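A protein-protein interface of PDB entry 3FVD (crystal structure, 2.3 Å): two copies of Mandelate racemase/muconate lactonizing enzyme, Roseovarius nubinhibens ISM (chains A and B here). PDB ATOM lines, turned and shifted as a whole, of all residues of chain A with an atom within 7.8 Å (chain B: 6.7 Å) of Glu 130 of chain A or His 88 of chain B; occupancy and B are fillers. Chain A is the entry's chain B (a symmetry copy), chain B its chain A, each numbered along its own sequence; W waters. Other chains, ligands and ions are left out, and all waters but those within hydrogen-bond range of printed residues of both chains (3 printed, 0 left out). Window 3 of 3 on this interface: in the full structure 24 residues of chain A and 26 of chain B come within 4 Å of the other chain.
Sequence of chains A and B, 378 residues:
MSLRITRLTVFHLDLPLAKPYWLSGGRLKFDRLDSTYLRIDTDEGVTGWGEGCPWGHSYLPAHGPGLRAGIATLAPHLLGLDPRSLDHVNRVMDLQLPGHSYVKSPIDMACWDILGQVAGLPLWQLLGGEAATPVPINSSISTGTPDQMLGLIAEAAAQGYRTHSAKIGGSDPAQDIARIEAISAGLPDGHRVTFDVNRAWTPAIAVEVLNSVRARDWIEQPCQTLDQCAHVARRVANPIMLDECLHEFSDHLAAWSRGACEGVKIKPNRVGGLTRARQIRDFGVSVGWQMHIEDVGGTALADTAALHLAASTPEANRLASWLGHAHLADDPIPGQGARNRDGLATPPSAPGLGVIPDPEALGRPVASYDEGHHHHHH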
ATOM      1  N   TRP A 124     -20.032  20.438  26.441  1.00  0.00           N
ATOM      2  CA  TRP A 124     -19.499  21.684  25.881  1.00  0.00           C
ATOM      3  C   TRP A 124     -18.086  21.509  25.281  1.00  0.00           C
ATOM      4  O   TRP A 124     -17.717  22.235  24.348  1.00  0.00           O
ATOM      5  CB  TRP A 124     -19.536  22.873  26.864  1.00  0.00           C
ATOM      6  CG  TRP A 124     -18.721  22.660  28.130  1.00  0.00           C
ATOM      7  CD1 TRP A 124     -19.219  22.243  29.351  1.00  0.00           C
ATOM      8  CD2 TRP A 124     -17.310  22.819  28.306  1.00  0.00           C
ATOM      9  NE1 TRP A 124     -18.204  22.164  30.263  1.00  0.00           N
ATOM     10  CE2 TRP A 124     -17.023  22.527  29.664  1.00  0.00           C
ATOM     11  CE3 TRP A 124     -16.267  23.192  27.468  1.00  0.00           C
ATOM     12  CZ2 TRP A 124     -15.727  22.565  30.193  1.00  0.00           C
ATOM     13  CZ3 TRP A 124     -14.990  23.238  27.986  1.00  0.00           C
ATOM     14  CH2 TRP A 124     -14.726  22.913  29.353  1.00  0.00           C
ATOM     15  N   GLN A 125     -17.305  20.544  25.772  1.00  0.00           N
ATOM     16  CA  GLN A 125     -15.995  20.409  25.195  1.00  0.00           C
ATOM     17  C   GLN A 125     -16.027  19.579  23.905  1.00  0.00           C
ATOM     18  O   GLN A 125     -15.328  19.902  22.954  1.00  0.00           O
ATOM     19  CB  GLN A 125     -15.011  19.834  26.159  1.00  0.00           C
ATOM     20  CG  GLN A 125     -13.643  19.874  25.610  1.00  0.00           C
ATOM     21  CD  GLN A 125     -12.622  19.774  26.751  1.00  0.00           C
ATOM     22  OE1 GLN A 125     -12.814  18.970  27.670  1.00  0.00           O
ATOM     23  NE2 GLN A 125     -11.563  20.588  26.712  1.00  0.00           N
ATOM     24  N   LEU A 127     -18.418  19.592  22.036  1.00  0.00           N
ATOM     25  CA  LEU A 127     -18.963  20.556  21.112  1.00  0.00           C
ATOM     26  C   LEU A 127     -18.002  21.649  20.766  1.00  0.00           C
ATOM     27  O   LEU A 127     -18.372  22.604  20.136  1.00  0.00           O
ATOM     28  CB  LEU A 127     -20.285  21.144  21.609  1.00  0.00           C
ATOM     29  CG  LEU A 127     -21.348  20.059  21.686  1.00  0.00           C
ATOM     30  CD1 LEU A 127     -22.514  20.527  22.563  1.00  0.00           C
ATOM     31  CD2 LEU A 127     -21.794  19.612  20.275  1.00  0.00           C
ATOM     32  N   GLY A 128     -16.768  21.521  21.166  1.00  0.00           N
ATOM     33  CA  GLY A 128     -15.764  22.450  20.709  1.00  0.00           C
ATOM     34  C   GLY A 128     -15.465  23.665  21.576  1.00  0.00           C
ATOM     35  O   GLY A 128     -14.607  24.494  21.197  1.00  0.00           O
ATOM     36  N   GLY A 129     -16.158  23.813  22.706  1.00  0.00           N
ATOM     37  CA  GLY A 129     -15.988  25.037  23.503  1.00  0.00           C
ATOM     38  C   GLY A 129     -14.673  25.064  24.286  1.00  0.00           C
ATOM     39  O   GLY A 129     -14.206  24.013  24.764  1.00  0.00           O
ATOM     40  N   GLU A 130     -14.073  26.250  24.441  1.00  0.00           N
ATOM     41  CA  GLU A 130     -12.850  26.339  25.294  1.00  0.00           C
ATOM     42  C   GLU A 130     -13.098  26.207  26.783  1.00  0.00           C
ATOM     43  O   GLU A 130     -12.192  25.796  27.495  1.00  0.00           O
ATOM     44  CB  GLU A 130     -11.961  27.608  25.022  1.00  0.00           C
ATOM     45  CG  GLU A 130     -12.584  28.972  25.276  1.00  0.00           C
ATOM     46  CD  GLU A 130     -11.546  30.098  25.457  1.00  0.00           C
ATOM     47  OE1 GLU A 130     -11.929  31.249  25.136  1.00  0.00           O
ATOM     48  OE2 GLU A 130     -10.398  29.853  25.949  1.00  0.00           O
ATOM     49  N   ALA A 131     -14.290  26.584  27.262  1.00  0.00           N
ATOM     50  CA  ALA A 131     -14.567  26.570  28.691  1.00  0.00           C
ATOM     51  C   ALA A 131     -16.041  26.544  28.964  1.00  0.00           C
ATOM     52  O   ALA A 131     -16.856  26.815  28.083  1.00  0.00           O
ATOM     53  CB  ALA A 131     -13.937  27.814  29.361  1.00  0.00           C
ATOM     54  N   ALA A 132     -16.382  26.241  30.199  1.00  0.00           N
ATOM     55  CA  ALA A 132     -17.782  26.270  30.647  1.00  0.00           C
ATOM     56  C   ALA A 132     -18.265  27.727  30.762  1.00  0.00           C
ATOM     57  O   ALA A 132     -18.380  28.293  31.835  1.00  0.00           O
ATOM     58  CB  ALA A 132     -17.910  25.473  31.985  1.00  0.00           C
ATOM     59  N   THR A 133     -18.518  28.355  29.632  1.00  0.00           N
ATOM     60  CA  THR A 133     -18.794  29.792  29.629  1.00  0.00           C
ATOM     61  C   THR A 133     -20.146  30.037  30.287  1.00  0.00           C
ATOM     62  O   THR A 133     -21.128  29.421  29.875  1.00  0.00           O
ATOM     63  CB  THR A 133     -18.789  30.353  28.166  1.00  0.00           C
ATOM     64  OG1 THR A 133     -17.519  30.077  27.555  1.00  0.00           O
ATOM     65  CG2 THR A 133     -19.001  31.829  28.138  1.00  0.00           C
ATOM     66  N   ALA A 311     -22.985  27.304  25.388  1.00  0.00           N
ATOM     67  CA  ALA A 311     -21.698  27.728  25.958  1.00  0.00           C
ATOM     68  C   ALA A 311     -20.529  27.521  24.938  1.00  0.00           C
ATOM     69  O   ALA A 311     -19.506  28.237  24.905  1.00  0.00           O
ATOM     70  CB  ALA A 311     -21.440  26.961  27.274  1.00  0.00           C
ATOM     71  N   SER A 312     -20.666  26.537  24.092  1.00  0.00           N
ATOM     72  CA  SER A 312     -19.586  26.268  23.139  1.00  0.00           C
ATOM     73  C   SER A 312     -19.675  27.177  21.910  1.00  0.00           C
ATOM     74  O   SER A 312     -18.854  27.079  21.003  1.00  0.00           O
ATOM     75  CB  SER A 312     -19.598  24.777  22.743  1.00  0.00           C
ATOM     76  OG  SER A 312     -20.835  24.393  22.142  1.00  0.00           O
ATOM     77  N   THR A 313     -20.699  28.022  21.839  1.00  0.00           N
ATOM     78  CA  THR A 313     -20.846  28.893  20.690  1.00  0.00           C
ATOM     79  C   THR A 313     -20.001  30.158  20.890  1.00  0.00           C
ATOM     80  O   THR A 313     -20.068  30.773  21.967  1.00  0.00           O
ATOM     81  CB  THR A 313     -22.304  29.217  20.469  1.00  0.00           C
ATOM     82  OG1 THR A 313     -23.034  27.993  20.281  1.00  0.00           O
ATOM     83  CG2 THR A 313     -22.542  30.128  19.289  1.00  0.00           C
ATOM     84  N   PRO A 314     -19.230  30.563  19.849  1.00  0.00           N
ATOM     85  CA  PRO A 314     -18.403  31.789  19.906  1.00  0.00           C
ATOM     86  C   PRO A 314     -19.274  32.973  20.292  1.00  0.00           C
ATOM     87  O   PRO A 314     -20.457  33.092  19.848  1.00  0.00           O
ATOM     88  CB  PRO A 314     -17.936  31.990  18.457  1.00  0.00           C
ATOM     89  CG  PRO A 314     -18.088  30.621  17.819  1.00  0.00           C
ATOM     90  CD  PRO A 314     -19.314  30.040  18.471  1.00  0.00           C
ATOM     91  N   LEU B  81      -2.833  25.776  24.652  1.00  0.00           N
ATOM     92  CA  LEU B  81      -4.227  25.552  24.350  1.00  0.00           C
ATOM     93  C   LEU B  81      -4.582  24.128  24.728  1.00  0.00           C
ATOM     94  O   LEU B  81      -3.740  23.205  24.647  1.00  0.00           O
ATOM     95  CB  LEU B  81      -4.511  25.737  22.845  1.00  0.00           C
ATOM     96  CG  LEU B  81      -4.368  27.084  22.150  1.00  0.00           C
ATOM     97  CD1 LEU B  81      -4.920  26.998  20.657  1.00  0.00           C
ATOM     98  CD2 LEU B  81      -5.081  28.179  23.007  1.00  0.00           C
ATOM     99  N   ASP B  82      -5.840  23.957  25.105  1.00  0.00           N
ATOM    100  CA  ASP B  82      -6.424  22.666  25.306  1.00  0.00           C
ATOM    101  C   ASP B  82      -6.799  22.064  23.950  1.00  0.00           C
ATOM    102  O   ASP B  82      -7.796  22.490  23.343  1.00  0.00           O
ATOM    103  CB  ASP B  82      -7.688  22.817  26.157  1.00  0.00           C
ATOM    104  CG  ASP B  82      -8.225  21.494  26.629  1.00  0.00           C
ATOM    105  OD1 ASP B  82      -7.838  20.450  26.028  1.00  0.00           O
ATOM    106  OD2 ASP B  82      -9.007  21.498  27.625  1.00  0.00           O
ATOM    107  N   SER B  85     -10.343  20.820  22.601  1.00  0.00           N
ATOM    108  CA  SER B  85     -11.374  21.788  22.198  1.00  0.00           C
ATOM    109  C   SER B  85     -11.176  22.199  20.715  1.00  0.00           C
ATOM    110  O   SER B  85     -10.589  23.253  20.418  1.00  0.00           O
ATOM    111  CB  SER B  85     -11.275  22.988  23.125  1.00  0.00           C
ATOM    112  OG  SER B  85     -11.869  22.684  24.371  1.00  0.00           O
ATOM    113  N   LEU B  86     -11.586  21.339  19.785  1.00  0.00           N
ATOM    114  CA  LEU B  86     -11.076  21.473  18.388  1.00  0.00           C
ATOM    115  C   LEU B  86     -11.567  22.734  17.656  1.00  0.00           C
ATOM    116  O   LEU B  86     -10.795  23.389  16.966  1.00  0.00           O
ATOM    117  CB  LEU B  86     -11.355  20.217  17.564  1.00  0.00           C
ATOM    118  CG  LEU B  86     -10.711  18.950  18.109  1.00  0.00           C
ATOM    119  CD1 LEU B  86     -11.454  17.751  17.536  1.00  0.00           C
ATOM    120  CD2 LEU B  86      -9.291  18.908  17.706  1.00  0.00           C
ATOM    121  N   ASP B  87     -12.839  23.060  17.810  1.00  0.00           N
ATOM    122  CA  ASP B  87     -13.417  24.263  17.243  1.00  0.00           C
ATOM    123  C   ASP B  87     -12.702  25.478  17.823  1.00  0.00           C
ATOM    124  O   ASP B  87     -12.398  26.398  17.117  1.00  0.00           O
ATOM    125  CB  ASP B  87     -14.899  24.366  17.599  1.00  0.00           C
ATOM    126  CG  ASP B  87     -15.747  23.210  17.028  1.00  0.00           C
ATOM    127  OD1 ASP B  87     -15.407  22.009  17.170  1.00  0.00           O
ATOM    128  OD2 ASP B  87     -16.827  23.481  16.499  1.00  0.00           O
ATOM    129  N   HIS B  88     -12.409  25.471  19.115  1.00  0.00           N
ATOM    130  CA  HIS B  88     -11.664  26.594  19.689  1.00  0.00           C
ATOM    131  C   HIS B  88     -10.243  26.721  19.104  1.00  0.00           C
ATOM    132  O   HIS B  88      -9.812  27.807  18.736  1.00  0.00           O
ATOM    133  CB  HIS B  88     -11.590  26.499  21.229  1.00  0.00           C
ATOM    134  CG  HIS B  88     -10.803  27.621  21.853  1.00  0.00           C
ATOM    135  ND1 HIS B  88      -9.552  27.441  22.427  1.00  0.00           N
ATOM    136  CD2 HIS B  88     -11.076  28.940  21.936  1.00  0.00           C
ATOM    137  CE1 HIS B  88      -9.112  28.604  22.870  1.00  0.00           C
ATOM    138  NE2 HIS B  88     -10.017  29.528  22.573  1.00  0.00           N
ATOM    139  N   VAL B  89      -9.511  25.620  19.064  1.00  0.00           N
ATOM    140  CA  VAL B  89      -8.222  25.628  18.369  1.00  0.00           C
ATOM    141  C   VAL B  89      -8.343  26.226  16.946  1.00  0.00           C
ATOM    142  O   VAL B  89      -7.599  27.118  16.602  1.00  0.00           O
ATOM    143  CB  VAL B  89      -7.546  24.210  18.397  1.00  0.00           C
ATOM    144  CG1 VAL B  89      -6.160  24.277  17.753  1.00  0.00           C
ATOM    145  CG2 VAL B  89      -7.426  23.662  19.864  1.00  0.00           C
ATOM    146  N   ASN B  90      -9.302  25.775  16.129  1.00  0.00           N
ATOM    147  CA  ASN B  90      -9.457  26.343  14.807  1.00  0.00           C
ATOM    148  C   ASN B  90      -9.770  27.860  14.809  1.00  0.00           C
ATOM    149  O   ASN B  90      -9.295  28.610  13.939  1.00  0.00           O
ATOM    150  CB  ASN B  90     -10.527  25.561  14.037  1.00  0.00           C
ATOM    151  CG  ASN B  90     -10.021  24.211  13.601  1.00  0.00           C
ATOM    152  OD1 ASN B  90      -9.676  24.038  12.442  1.00  0.00           O
ATOM    153  ND2 ASN B  90      -9.880  23.274  14.544  1.00  0.00           N
ATOM    154  N   ARG B  91     -10.559  28.312  15.784  1.00  0.00           N
ATOM    155  CA  ARG B  91     -10.904  29.728  15.829  1.00  0.00           C
ATOM    156  C   ARG B  91      -9.663  30.550  16.057  1.00  0.00           C
ATOM    157  O   ARG B  91      -9.558  31.627  15.462  1.00  0.00           O
ATOM    158  CB  ARG B  91     -11.920  30.058  16.919  1.00  0.00           C
ATOM    159  CG  ARG B  91     -13.328  29.886  16.426  1.00  0.00           C
ATOM    160  CD  ARG B  91     -14.358  30.396  17.503  1.00  0.00           C
ATOM    161  NE  ARG B  91     -14.373  29.515  18.696  1.00  0.00           N
ATOM    162  CZ  ARG B  91     -15.053  28.365  18.869  1.00  0.00           C
ATOM    163  NH1 ARG B  91     -15.859  27.821  17.913  1.00  0.00           N
ATOM    164  NH2 ARG B  91     -14.927  27.743  20.047  1.00  0.00           N
ATOM    165  N   VAL B  92      -8.738  30.008  16.866  1.00  0.00           N
ATOM    166  CA  VAL B  92      -7.544  30.711  17.280  1.00  0.00           C
ATOM    167  C   VAL B  92      -6.611  30.750  16.065  1.00  0.00           C
ATOM    168  O   VAL B  92      -6.037  31.793  15.751  1.00  0.00           O
ATOM    169  CB  VAL B  92      -6.851  30.019  18.482  1.00  0.00           C
ATOM    170  CG1 VAL B  92      -5.420  30.506  18.628  1.00  0.00           C
ATOM    171  CG2 VAL B  92      -7.603  30.297  19.777  1.00  0.00           C
ATOM    172  N   MET B  93      -6.497  29.625  15.355  1.00  0.00           N
ATOM    173  CA  MET B  93      -5.714  29.580  14.122  1.00  0.00           C
ATOM    174  C   MET B  93      -6.287  30.576  13.127  1.00  0.00           C
ATOM    175  O   MET B  93      -5.515  31.290  12.493  1.00  0.00           O
ATOM    176  CB  MET B  93      -5.655  28.194  13.493  1.00  0.00           C
ATOM    177  CG  MET B  93      -4.809  27.209  14.335  1.00  0.00           C
ATOM    178  SD  MET B  93      -4.461  25.659  13.459  1.00  0.00           S
ATOM    179  CE  MET B  93      -6.100  24.930  13.422  1.00  0.00           C
HETATM  180  O   HOH W   1     -17.566  25.772  18.879  1.00  0.00           O
HETATM  181  O   HOH W   2     -15.129  28.782  22.698  1.00  0.00           O
HETATM  182  O   HOH W   3     -13.808  18.999  20.540  1.00  0.00           O
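Water W1 lies within hydrogen-bond range of O of Ser 312 of chain A (2.8 Å), NH1 of Arg 91 of chain B (2.8 Å) and OD2 of Asp 87 of chain B (3.4 Å). Water W2 bridges the guanidinium group of Arg 91 of chain B and the backbone NH of Glu 130 of chain A. Water W3 lies within hydrogen-bond range of the backbone carbonyl oxygen (O) of Gln 125 of chain A (3.0 Å) and the backbone NH (N) of Leu 86 of chain B (3.3 Å).
CA of Gly 128 of chain A touches OD1 of Asp 87 of chain B, 3.6 Å away. Glu 130 of chain A touches Ser 85 of chain B. CG of Pro 314 of chain A touches NH1 of Arg 91 of chain B (3.6 Å).
OD2 of Asp 82 of chain B is in hydrogen-bond range of NE2 of Gln 125 of chain A (2.9 Å). OG of Ser 85 of chain B lies within hydrogen-bond range of NE2 of Gln 125 of chain A, at 3.2 Å. The side-chain hydroxyl (OG) of Ser 85 of chain B lies within hydrogen-bond range of the backbone carbonyl oxygen (O) of Gly 129 of chain A, at 2.7 Å. O of Gly 128 of chain A is in hydrogen-bond range of N of His 88 of chain B (3.2 Å). NE2 of His 88 of chain B sits close to OE2 of Glu 130 of chain A (3.4 Å). O of Gly 128 of chain A lies within hydrogen-bond range of NH2 of Arg 91 of chain B.
Along chain B the printed residues that touch a printed residue of chain A span positions 82 to 91. Printed residues of chain A that touch a printed residue of chain B: Gln 125, Gly 128, Gly 129, Glu 130 and Pro 314. Among the printed residues, 9 pairs touch across the chains. Among the printed residues, no Asp or Glu carboxylate lies within 4 Å of a Lys or Arg side-chain nitrogen of the other chain.
Of chain B, only Ser 85 and His 88 come within 4 Å of Glu 130 of chain A. His 88 of chain B touches just these residues of chain A: Gly 128 (3.2 Å) and Glu 130 (3.3 Å). Printed residues of chain B within 4 Å of Gly 128 of chain A: Asp 87 (3.6 Å), His 88 (3.2 Å) and Arg 91 (3.5 Å). Printed residues of chain A within 4 Å of Arg 91 of chain B: Gly 128 and Pro 314. The nearest residue of chain B that does not touch Glu 130 of chain A is Arg 91 of chain B (4.7 Å).
No position is printed for both chains.
N of Gly 129 of chain A sits at hydrogen-bond distance from O of Trp 124 of chain A.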
